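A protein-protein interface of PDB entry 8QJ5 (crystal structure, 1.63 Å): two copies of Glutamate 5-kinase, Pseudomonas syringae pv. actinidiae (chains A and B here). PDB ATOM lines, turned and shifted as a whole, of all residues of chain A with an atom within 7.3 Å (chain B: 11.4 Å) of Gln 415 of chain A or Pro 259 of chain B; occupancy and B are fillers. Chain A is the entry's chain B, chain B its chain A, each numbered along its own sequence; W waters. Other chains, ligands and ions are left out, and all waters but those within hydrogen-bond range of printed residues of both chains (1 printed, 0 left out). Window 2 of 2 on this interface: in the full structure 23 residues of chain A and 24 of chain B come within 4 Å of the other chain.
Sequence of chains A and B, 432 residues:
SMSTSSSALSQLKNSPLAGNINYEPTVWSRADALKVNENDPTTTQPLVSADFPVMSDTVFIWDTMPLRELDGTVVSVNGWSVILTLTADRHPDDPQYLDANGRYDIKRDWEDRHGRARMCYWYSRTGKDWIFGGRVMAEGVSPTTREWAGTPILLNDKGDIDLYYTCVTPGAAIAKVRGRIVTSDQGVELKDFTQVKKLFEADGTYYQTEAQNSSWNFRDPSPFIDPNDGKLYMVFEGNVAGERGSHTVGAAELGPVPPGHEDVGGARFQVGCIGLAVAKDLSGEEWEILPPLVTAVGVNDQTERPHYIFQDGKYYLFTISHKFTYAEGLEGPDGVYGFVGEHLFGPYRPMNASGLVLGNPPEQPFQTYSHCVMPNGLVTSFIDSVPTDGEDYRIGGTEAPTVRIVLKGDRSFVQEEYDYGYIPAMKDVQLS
No position is printed for both chains.
Of the 14 pairs that touch across the chains among the printed residues, none has its exchanged pair printed and touching as well.
OE1 of Gln 415 of chain A sits close to O of Pro 256 of chain B (3.4 Å).
O of Val 257 of chain B sits close to OE1 of Gln 415 of chain A, at 3.0 Å.
OG1 of Thr 42 of chain A sits at hydrogen-bond distance from NZ of Lys 35 of chain B (2.8 Å).
O of Phe 413 of chain A lies within hydrogen-bond range of N of Val 406 of chain A (2.9 Å).
N of Ala 31 of chain B lies close to OG of Ser 29 of chain B, 3.3 Å away.
O of Arg 404 of chain A lies within hydrogen-bond range of N of Gln 415 of chain A (2.8 Å).
The backbone carbonyl oxygen of Thr 42 of chain A sits at hydrogen-bond distance from the backbone NH of Val 414 of chain A, at 2.9 Å.
The backbone NH of Ala 31 of chain B is in hydrogen-bond range of the backbone carbonyl oxygen of Leu 254 of chain B (2.9 Å).
The backbone NH of Ser 29 of chain B lies within hydrogen-bond range of the side-chain carboxylate of Asp 32 of chain B (3.0 Å).
Of the 15 printed residues of chain A, 6 touch a printed residue of chain B.
Hydrophobic or aromatic side chains of chain A within 4 Å of the printed part of chain B: Pro 41, Val 406, Phe 413 and Val 414.
Hydrophobic or aromatic side chains of chain B within 4 Å of the printed part of chain A: Ala 31, Pro 256, Pro 258, Pro 259 and His 261.
Among the printed residues, 14 pairs touch across the chains.
Water W1 bridges the backbone carbonyl oxygen (O) of Val 414 of chain A (2.8 Å) and the backbone carbonyl oxygen (O) of Pro 256 of chain B (2.9 Å).
Printed residues of chain B within 4 Å of Pro 41 of chain A: Leu 34, Pro 258 and His 261.
Of the printed residues of chain B, Thr 42 of chain A touches Ala 31 (3.7 Å) and Lys 35 (2.8 Å).
No residue of chain B comes within 4 Å of Arg 404 of chain A.
Val 406 of chain A touches just one residue of chain B: Pro 256.
Of chain B, only Pro 258 (3.6 Å) comes within 4 Å of Val 414 of chain A.
Of chain B, only Pro 256 (3.4 Å), Val 257 (3.0 Å) and Pro 259 (3.6 Å) come within 4 Å of Gln 415 of chain A.
Of the printed residues of chain A, Asp 32 of chain B touches Phe 413 (3.8 Å).
Printed residues of chain A within 4 Å of Pro 256 of chain B: Val 406, Phe 413 and Gln 415.
Of the printed residues of chain A, Val 257 of chain B touches Gln 415.
Pro 259 of chain B touches just one residue of chain A: Gln 415 (3.6 Å).
The nearest residue of chain A that does not touch Pro 259 of chain B is Val 414 of chain A (4.4 Å).
The nearest printed residue of chain A that does not touch Lys 35 of chain B is Pro 41 of chain A (5.6 Å).
Among the printed residues, merely in contact across the chains: Pro 41 of chain A with Leu 34 of chain B, Pro 41 of chain A with Pro 258 of chain B, Pro 41 of chain A with His 261 of chain B, Thr 42 of chain A with Ala 31 of chain B, Val 406 of chain A with Pro 256 of chain B, Phe 413 of chain A with Ala 31 of chain B, Phe 413 of chain A with Asp 32 of chain B, Phe 413 of chain A with Lys 35 of chain B, Phe 413 of chain A with Pro 256 of chain B, Val 414 of chain A with Pro 258 of chain B and Gln 415 of chain A with Pro 259 of chain B.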
ATOM      1  N   PRO A  41      23.291  11.177   6.227  1.00  0.00           N
ATOM      2  CA  PRO A  41      24.743  11.177   6.058  1.00  0.00           C
ATOM      3  C   PRO A  41      25.167  10.987   4.606  1.00  0.00           C
ATOM      4  O   PRO A  41      26.300  11.365   4.275  1.00  0.00           O
ATOM      5  CB  PRO A  41      25.229   9.939   6.851  1.00  0.00           C
ATOM      6  CG  PRO A  41      24.006   9.079   6.981  1.00  0.00           C
ATOM      7  CD  PRO A  41      22.790   9.996   6.961  1.00  0.00           C
ATOM      8  N   THR A  42      24.272  10.479   3.744  1.00  0.00           N
ATOM      9  CA  THR A  42      24.577  10.300   2.339  1.00  0.00           C
ATOM     10  C   THR A  42      24.469  11.615   1.545  1.00  0.00           C
ATOM     11  O   THR A  42      24.911  11.636   0.394  1.00  0.00           O
ATOM     12  CB  THR A  42      23.678   9.251   1.672  1.00  0.00           C
ATOM     13  OG1 THR A  42      22.338   9.757   1.549  1.00  0.00           O
ATOM     14  CG2 THR A  42      23.658   7.904   2.371  1.00  0.00           C
ATOM     15  N   THR A  44      25.151  14.875   3.132  1.00  0.00           N
ATOM     16  CA  THR A  44      25.678  15.959   3.963  1.00  0.00           C
ATOM     17  C   THR A  44      27.122  16.251   3.536  1.00  0.00           C
ATOM     18  O   THR A  44      27.951  15.322   3.434  1.00  0.00           O
ATOM     19  CB  THR A  44      25.576  15.647   5.461  1.00  0.00           C
ATOM     20  OG1 THR A  44      24.189  15.450   5.761  1.00  0.00           O
ATOM     21  CG2 THR A  44      26.019  16.827   6.315  1.00  0.00           C
ATOM     22  N   PRO A  46      30.936  17.285   4.149  1.00  0.00           N
ATOM     23  CA  PRO A  46      31.843  17.160   5.291  1.00  0.00           C
ATOM     24  C   PRO A  46      32.086  18.492   6.007  1.00  0.00           C
ATOM     25  O   PRO A  46      32.030  19.524   5.380  1.00  0.00           O
ATOM     26  CB  PRO A  46      33.184  16.689   4.663  1.00  0.00           C
ATOM     27  CG  PRO A  46      32.995  16.686   3.138  1.00  0.00           C
ATOM     28  CD  PRO A  46      31.494  16.743   2.893  1.00  0.00           C
ATOM     29  N   LEU A 358      23.303  17.714  -1.818  1.00  0.00           N
ATOM     30  CA  LEU A 358      24.339  17.850  -0.804  1.00  0.00           C
ATOM     31  C   LEU A 358      24.035  19.095   0.020  1.00  0.00           C
ATOM     32  O   LEU A 358      24.148  20.228  -0.461  1.00  0.00           O
ATOM     33  CB  LEU A 358      25.669  17.992  -1.559  1.00  0.00           C
ATOM     34  CG  LEU A 358      26.954  17.747  -0.774  1.00  0.00           C
ATOM     35  CD1 LEU A 358      27.098  16.265  -0.389  1.00  0.00           C
ATOM     36  CD2 LEU A 358      28.158  18.171  -1.636  1.00  0.00           C
ATOM     37  N   VAL A 403      34.639  17.708  -2.662  1.00  0.00           N
ATOM     38  CA  VAL A 403      34.106  16.416  -2.221  1.00  0.00           C
ATOM     39  C   VAL A 403      33.530  15.687  -3.431  1.00  0.00           C
ATOM     40  O   VAL A 403      33.019  16.336  -4.324  1.00  0.00           O
ATOM     41  CB  VAL A 403      33.092  16.605  -1.061  1.00  0.00           C
ATOM     42  CG1 VAL A 403      31.800  17.266  -1.510  1.00  0.00           C
ATOM     43  CG2 VAL A 403      32.722  15.259  -0.416  1.00  0.00           C
ATOM     44  N   ARG A 404      33.590  14.341  -3.486  1.00  0.00           N
ATOM     45  CA  ARG A 404      33.090  13.613  -4.638  1.00  0.00           C
ATOM     46  C   ARG A 404      31.716  13.044  -4.243  1.00  0.00           C
ATOM     47  O   ARG A 404      31.489  12.758  -3.059  1.00  0.00           O
ATOM     48  CB  ARG A 404      34.012  12.419  -4.962  1.00  0.00           C
ATOM     49  CG  ARG A 404      33.602  11.723  -6.255  1.00  0.00           C
ATOM     50  CD  ARG A 404      34.609  10.699  -6.804  1.00  0.00           C
ATOM     51  NE  ARG A 404      34.760   9.676  -5.792  1.00  0.00           N
ATOM     52  CZ  ARG A 404      34.074   8.526  -5.794  1.00  0.00           C
ATOM     53  NH1 ARG A 404      33.218   8.261  -6.763  1.00  0.00           N
ATOM     54  NH2 ARG A 404      34.284   7.647  -4.850  1.00  0.00           N
ATOM     55  N   ILE A 405      30.783  13.093  -5.185  1.00  0.00           N
ATOM     56  CA  ILE A 405      29.512  12.376  -5.019  1.00  0.00           C
ATOM     57  C   ILE A 405      29.432  11.342  -6.138  1.00  0.00           C
ATOM     58  O   ILE A 405      30.005  11.538  -7.214  1.00  0.00           O
ATOM     59  CB  ILE A 405      28.319  13.373  -5.058  1.00  0.00           C
ATOM     60  CG1 ILE A 405      28.063  13.918  -6.476  1.00  0.00           C
ATOM     61  CG2 ILE A 405      28.437  14.435  -3.979  1.00  0.00           C
ATOM     62  CD1 ILE A 405      26.829  14.902  -6.557  1.00  0.00           C
ATOM     63  N   VAL A 406      28.636  10.281  -5.931  1.00  0.00           N
ATOM     64  CA  VAL A 406      28.338   9.358  -7.032  1.00  0.00           C
ATOM     65  C   VAL A 406      26.833   9.365  -7.260  1.00  0.00           C
ATOM     66  O   VAL A 406      26.058   9.578  -6.331  1.00  0.00           O
ATOM     67  CB  VAL A 406      28.806   7.919  -6.753  1.00  0.00           C
ATOM     68  CG1 VAL A 406      30.309   7.825  -6.595  1.00  0.00           C
ATOM     69  CG2 VAL A 406      28.122   7.325  -5.560  1.00  0.00           C
ATOM     70  N   PHE A 413      25.073   9.907  -3.565  1.00  0.00           N
ATOM     71  CA  PHE A 413      25.736   9.519  -2.320  1.00  0.00           C
ATOM     72  C   PHE A 413      27.053  10.300  -2.211  1.00  0.00           C
ATOM     73  O   PHE A 413      27.912  10.184  -3.078  1.00  0.00           O
ATOM     74  CB  PHE A 413      26.064   8.027  -2.516  1.00  0.00           C
ATOM     75  CG  PHE A 413      24.797   7.184  -2.566  1.00  0.00           C
ATOM     76  CD1 PHE A 413      24.230   6.745  -1.385  1.00  0.00           C
ATOM     77  CD2 PHE A 413      24.211   6.847  -3.780  1.00  0.00           C
ATOM     78  CE1 PHE A 413      23.068   5.959  -1.390  1.00  0.00           C
ATOM     79  CE2 PHE A 413      23.036   6.076  -3.796  1.00  0.00           C
ATOM     80  CZ  PHE A 413      22.513   5.613  -2.600  1.00  0.00           C
ATOM     81  N   VAL A 414      27.282  10.921  -1.051  1.00  0.00           N
ATOM     82  CA  VAL A 414      28.548  11.620  -0.821  1.00  0.00           C
ATOM     83  C   VAL A 414      29.646  10.584  -0.558  1.00  0.00           C
ATOM     84  O   VAL A 414      29.395   9.536   0.067  1.00  0.00           O
ATOM     85  CB  VAL A 414      28.434  12.686   0.284  1.00  0.00           C
ATOM     86  CG1 VAL A 414      28.286  12.079   1.671  1.00  0.00           C
ATOM     87  CG2 VAL A 414      29.662  13.648   0.245  1.00  0.00           C
ATOM     88  N   GLN A 415      30.859  10.882  -1.070  1.00  0.00           N
ATOM     89  CA  GLN A 415      32.046  10.014  -0.945  1.00  0.00           C
ATOM     90  C   GLN A 415      33.174  10.798  -0.248  1.00  0.00           C
ATOM     91  O   GLN A 415      32.916  11.571   0.702  1.00  0.00           O
ATOM     92  CB  GLN A 415      32.382   9.337  -2.275  1.00  0.00           C
ATOM     93  CG  GLN A 415      31.229   8.496  -2.853  1.00  0.00           C
ATOM     94  CD  GLN A 415      31.107   7.173  -2.112  1.00  0.00           C
ATOM     95  OE1 GLN A 415      30.520   7.060  -1.025  1.00  0.00           O
ATOM     96  NE2 GLN A 415      31.762   6.157  -2.655  1.00  0.00           N
ATOM     97  N   GLU A 416      34.414  10.617  -0.713  1.00  0.00           N
ATOM     98  CA  GLU A 416      35.556  11.173   0.003  1.00  0.00           C
ATOM     99  C   GLU A 416      35.778  12.664  -0.308  1.00  0.00           C
ATOM    100  O   GLU A 416      35.356  13.176  -1.346  1.00  0.00           O
ATOM    101  CB  GLU A 416      36.839  10.388  -0.324  1.00  0.00           C
ATOM    102  CG  GLU A 416      37.297  10.529  -1.762  1.00  0.00           C
ATOM    103  CD  GLU A 416      36.572   9.804  -2.874  1.00  0.00           C
ATOM    104  OE1 GLU A 416      35.683   8.950  -2.551  1.00  0.00           O
ATOM    105  OE2 GLU A 416      36.883  10.053  -4.050  1.00  0.00           O
ATOM    106  N   GLU A 417      36.512  13.307   0.600  1.00  0.00           N
ATOM    107  CA  GLU A 417      36.858  14.717   0.412  1.00  0.00           C
ATOM    108  C   GLU A 417      38.324  14.848   0.020  1.00  0.00           C
ATOM    109  O   GLU A 417      39.142  13.985   0.349  1.00  0.00           O
ATOM    110  CB  GLU A 417      36.474  15.566   1.628  1.00  0.00           C
ATOM    111  CG  GLU A 417      37.324  15.413   2.872  1.00  0.00           C
ATOM    112  CD  GLU A 417      36.839  16.323   3.999  1.00  0.00           C
ATOM    113  OE1 GLU A 417      36.773  17.574   3.804  1.00  0.00           O
ATOM    114  OE2 GLU A 417      36.435  15.770   5.050  1.00  0.00           O
ATOM    115  N   TYR A 418      38.614  15.973  -0.645  1.00  0.00           N
ATOM    116  CA  TYR A 418      39.906  16.340  -1.204  1.00  0.00           C
ATOM    117  C   TYR A 418      40.360  17.685  -0.640  1.00  0.00           C
ATOM    118  O   TYR A 418      39.748  18.258   0.275  1.00  0.00           O
ATOM    119  CB  TYR A 418      39.697  16.464  -2.715  1.00  0.00           C
ATOM    120  CG  TYR A 418      39.404  15.152  -3.383  1.00  0.00           C
ATOM    121  CD1 TYR A 418      38.141  14.565  -3.293  1.00  0.00           C
ATOM    122  CD2 TYR A 418      40.405  14.468  -4.048  1.00  0.00           C
ATOM    123  CE1 TYR A 418      37.878  13.339  -3.884  1.00  0.00           C
ATOM    124  CE2 TYR A 418      40.144  13.255  -4.680  1.00  0.00           C
ATOM    125  CZ  TYR A 418      38.882  12.692  -4.581  1.00  0.00           C
ATOM    126  OH  TYR A 418      38.628  11.510  -5.204  1.00  0.00           O
ATOM    127  N   SER B  29      20.593  -1.756  -0.515  1.00  0.00           N
ATOM    128  CA  SER B  29      21.888  -1.708   0.146  1.00  0.00           C
ATOM    129  C   SER B  29      21.828  -0.963   1.471  1.00  0.00           C
ATOM    130  O   SER B  29      20.869  -0.234   1.780  1.00  0.00           O
ATOM    131  CB  SER B  29      22.914  -1.042  -0.778  1.00  0.00           C
ATOM    132  OG  SER B  29      22.651   0.381  -0.822  1.00  0.00           O
ATOM    133  N   ARG B  30      22.928  -1.072   2.217  1.00  0.00           N
ATOM    134  CA  ARG B  30      23.071  -0.322   3.452  1.00  0.00           C
ATOM    135  C   ARG B  30      23.056   1.176   3.161  1.00  0.00           C
ATOM    136  O   ARG B  30      22.487   1.929   3.958  1.00  0.00           O
ATOM    137  CB  ARG B  30      24.376  -0.722   4.155  1.00  0.00           C
ATOM    138  CG  ARG B  30      24.286  -2.161   4.662  1.00  0.00           C
ATOM    139  CD  ARG B  30      25.550  -2.579   5.411  1.00  0.00           C
ATOM    140  NE  ARG B  30      25.856  -1.812   6.615  1.00  0.00           N
ATOM    141  CZ  ARG B  30      25.469  -2.054   7.869  1.00  0.00           C
ATOM    142  NH1 ARG B  30      24.652  -3.083   8.123  1.00  0.00           N
ATOM    143  NH2 ARG B  30      25.870  -1.226   8.844  1.00  0.00           N
ATOM    144  N   ALA B  31      23.718   1.602   2.061  1.00  0.00           N
ATOM    145  CA  ALA B  31      23.728   3.028   1.695  1.00  0.00           C
ATOM    146  C   ALA B  31      22.292   3.534   1.459  1.00  0.00           C
ATOM    147  O   ALA B  31      21.928   4.646   1.854  1.00  0.00           O
ATOM    148  CB  ALA B  31      24.587   3.258   0.462  1.00  0.00           C
ATOM    149  N   ASP B  32      21.468   2.700   0.816  1.00  0.00           N
ATOM    150  CA  ASP B  32      20.064   3.088   0.617  1.00  0.00           C
ATOM    151  C   ASP B  32      19.381   3.274   1.990  1.00  0.00           C
ATOM    152  O   ASP B  32      18.646   4.243   2.220  1.00  0.00           O
ATOM    153  CB  ASP B  32      19.266   2.014  -0.133  1.00  0.00           C
ATOM    154  CG  ASP B  32      19.669   1.745  -1.591  1.00  0.00           C
ATOM    155  OD1 ASP B  32      20.197   2.679  -2.296  1.00  0.00           O
ATOM    156  OD2 ASP B  32      19.530   0.559  -2.019  1.00  0.00           O
ATOM    157  N   LEU B  34      20.612   4.026   4.791  1.00  0.00           N
ATOM    158  CA  LEU B  34      21.038   5.164   5.593  1.00  0.00           C
ATOM    159  C   LEU B  34      20.235   6.437   5.258  1.00  0.00           C
ATOM    160  O   LEU B  34      20.285   7.397   6.027  1.00  0.00           O
ATOM    161  CB  LEU B  34      22.527   5.483   5.348  1.00  0.00           C
ATOM    162  CG  LEU B  34      23.517   4.457   5.949  1.00  0.00           C
ATOM    163  CD1 LEU B  34      24.948   4.785   5.431  1.00  0.00           C
ATOM    164  CD2 LEU B  34      23.508   4.568   7.495  1.00  0.00           C
ATOM    165  N   LYS B  35      19.533   6.424   4.133  1.00  0.00           N
ATOM    166  CA  LYS B  35      18.629   7.517   3.778  1.00  0.00           C
ATOM    167  C   LYS B  35      17.268   7.431   4.502  1.00  0.00           C
ATOM    168  O   LYS B  35      16.430   8.349   4.371  1.00  0.00           O
ATOM    169  CB  LYS B  35      18.345   7.438   2.269  1.00  0.00           C
ATOM    170  CG  LYS B  35      19.520   7.781   1.364  1.00  0.00           C
ATOM    171  CD  LYS B  35      19.037   7.866  -0.101  1.00  0.00           C
ATOM    172  CE  LYS B  35      20.192   8.162  -1.044  1.00  0.00           C
ATOM    173  NZ  LYS B  35      20.827   9.491  -0.767  1.00  0.00           N
ATOM    174  N   ALA B 251      30.615  -5.267  -1.549  1.00  0.00           N
ATOM    175  CA  ALA B 251      30.359  -3.952  -2.141  1.00  0.00           C
ATOM    176  C   ALA B 251      28.887  -3.724  -2.453  1.00  0.00           C
ATOM    177  O   ALA B 251      28.398  -2.594  -2.264  1.00  0.00           O
ATOM    178  CB  ALA B 251      31.174  -3.767  -3.400  1.00  0.00           C
ATOM    179  N   LEU B 254      26.844  -3.294   0.720  1.00  0.00           N
ATOM    180  CA  LEU B 254      27.142  -2.087   1.468  1.00  0.00           C
ATOM    181  C   LEU B 254      26.606  -0.866   0.718  1.00  0.00           C
ATOM    182  O   LEU B 254      26.054   0.063   1.316  1.00  0.00           O
ATOM    183  CB  LEU B 254      28.669  -1.966   1.481  1.00  0.00           C
ATOM    184  CG  LEU B 254      29.236  -0.847   2.354  1.00  0.00           C
ATOM    185  CD1 LEU B 254      28.830  -0.990   3.817  1.00  0.00           C
ATOM    186  CD2 LEU B 254      30.766  -0.842   2.271  1.00  0.00           C
ATOM    187  N   GLY B 255      26.769  -0.881  -0.618  1.00  0.00           N
ATOM    188  CA  GLY B 255      26.452   0.307  -1.395  1.00  0.00           C
ATOM    189  C   GLY B 255      27.457   1.440  -1.139  1.00  0.00           C
ATOM    190  O   GLY B 255      28.419   1.294  -0.373  1.00  0.00           O
ATOM    191  N   PRO B 256      27.194   2.629  -1.721  1.00  0.00           N
ATOM    192  CA  PRO B 256      28.115   3.769  -1.621  1.00  0.00           C
ATOM    193  C   PRO B 256      27.951   4.555  -0.326  1.00  0.00           C
ATOM    194  O   PRO B 256      27.466   5.712  -0.342  1.00  0.00           O
ATOM    195  CB  PRO B 256      27.765   4.654  -2.849  1.00  0.00           C
ATOM    196  CG  PRO B 256      26.478   4.122  -3.402  1.00  0.00           C
ATOM    197  CD  PRO B 256      26.141   2.804  -2.738  1.00  0.00           C
ATOM    198  N   VAL B 257      28.272   3.873   0.789  1.00  0.00           N
ATOM    199  CA  VAL B 257      28.174   4.458   2.110  1.00  0.00           C
ATOM    200  C   VAL B 257      29.131   5.633   2.199  1.00  0.00           C
ATOM    201  O   VAL B 257      30.209   5.592   1.594  1.00  0.00           O
ATOM    202  CB  VAL B 257      28.398   3.460   3.257  1.00  0.00           C
ATOM    203  CG1 VAL B 257      27.220   2.454   3.355  1.00  0.00           C
ATOM    204  CG2 VAL B 257      29.742   2.724   3.202  1.00  0.00           C
ATOM    205  N   PRO B 258      28.795   6.662   3.006  1.00  0.00           N
ATOM    206  CA  PRO B 258      29.711   7.799   3.187  1.00  0.00           C
ATOM    207  C   PRO B 258      30.828   7.405   4.157  1.00  0.00           C
ATOM    208  O   PRO B 258      30.739   6.406   4.857  1.00  0.00           O
ATOM    209  CB  PRO B 258      28.790   8.843   3.856  1.00  0.00           C
ATOM    210  CG  PRO B 258      27.714   8.049   4.564  1.00  0.00           C
ATOM    211  CD  PRO B 258      27.538   6.790   3.743  1.00  0.00           C
ATOM    212  N   PRO B 259      31.902   8.221   4.287  1.00  0.00           N
ATOM    213  CA  PRO B 259      32.947   7.985   5.285  1.00  0.00           C
ATOM    214  C   PRO B 259      32.420   7.788   6.697  1.00  0.00           C
ATOM    215  O   PRO B 259      31.518   8.487   7.142  1.00  0.00           O
ATOM    216  CB  PRO B 259      33.777   9.276   5.155  1.00  0.00           C
ATOM    217  CG  PRO B 259      33.650   9.588   3.677  1.00  0.00           C
ATOM    218  CD  PRO B 259      32.161   9.419   3.444  1.00  0.00           C
ATOM    219  N   GLY B 260      32.935   6.740   7.352  1.00  0.00           N
ATOM    220  CA  GLY B 260      32.612   6.498   8.739  1.00  0.00           C
ATOM    221  C   GLY B 260      31.456   5.520   8.894  1.00  0.00           C
ATOM    222  O   GLY B 260      31.007   5.319  10.018  1.00  0.00           O
ATOM    223  N   HIS B 261      30.956   4.989   7.762  1.00  0.00           N
ATOM    224  CA  HIS B 261      29.900   3.963   7.798  1.00  0.00           C
ATOM    225  C   HIS B 261      30.380   2.653   7.171  1.00  0.00           C
ATOM    226  O   HIS B 261      29.568   1.892   6.645  1.00  0.00           O
ATOM    227  CB  HIS B 261      28.643   4.527   7.106  1.00  0.00           C
ATOM    228  CG  HIS B 261      27.884   5.451   7.989  1.00  0.00           C
ATOM    229  ND1 HIS B 261      28.109   6.825   8.025  1.00  0.00           N
ATOM    230  CD2 HIS B 261      26.923   5.203   8.903  1.00  0.00           C
ATOM    231  CE1 HIS B 261      27.302   7.392   8.913  1.00  0.00           C
ATOM    232  NE2 HIS B 261      26.570   6.412   9.473  1.00  0.00           N
ATOM    233  N   GLU B 262      31.671   2.328   7.300  1.00  0.00           N
ATOM    234  CA  GLU B 262      32.195   1.091   6.716  1.00  0.00           C
ATOM    235  C   GLU B 262      31.991  -0.168   7.574  1.00  0.00           C
ATOM    236  O   GLU B 262      32.120  -1.281   7.054  1.00  0.00           O
ATOM    237  CB  GLU B 262      33.680   1.229   6.358  1.00  0.00           C
ATOM    238  CG  GLU B 262      33.949   2.281   5.293  1.00  0.00           C
ATOM    239  CD  GLU B 262      34.222   3.666   5.858  1.00  0.00           C
ATOM    240  OE1 GLU B 262      33.887   3.884   7.062  1.00  0.00           O
ATOM    241  OE2 GLU B 262      34.755   4.532   5.102  1.00  0.00           O
ATOM    242  N   ASP B 263      31.711  -0.032   8.876  1.00  0.00           N
ATOM    243  CA  ASP B 263      31.669  -1.173   9.768  1.00  0.00           C
ATOM    244  C   ASP B 263      30.282  -1.803   9.650  1.00  0.00           C
ATOM    245  O   ASP B 263      29.270  -1.113   9.745  1.00  0.00           O
ATOM    246  CB  ASP B 263      31.958  -0.764  11.216  1.00  0.00           C
ATOM    247  CG  ASP B 263      32.286  -1.906  12.179  1.00  0.00           C
ATOM    248  OD1 ASP B 263      32.009  -3.104  11.849  1.00  0.00           O
ATOM    249  OD2 ASP B 263      32.831  -1.612  13.280  1.00  0.00           O
ATOM    250  N   GLY B 329      24.083  -0.880  12.823  1.00  0.00           N
ATOM    251  CA  GLY B 329      24.602   0.257  12.077  1.00  0.00           C
ATOM    252  C   GLY B 329      23.520   0.969  11.257  1.00  0.00           C
ATOM    253  O   GLY B 329      23.800   2.013  10.666  1.00  0.00           O
HETATM  254  O   HOH W   1      26.986   8.334   0.854  1.00  0.00           O
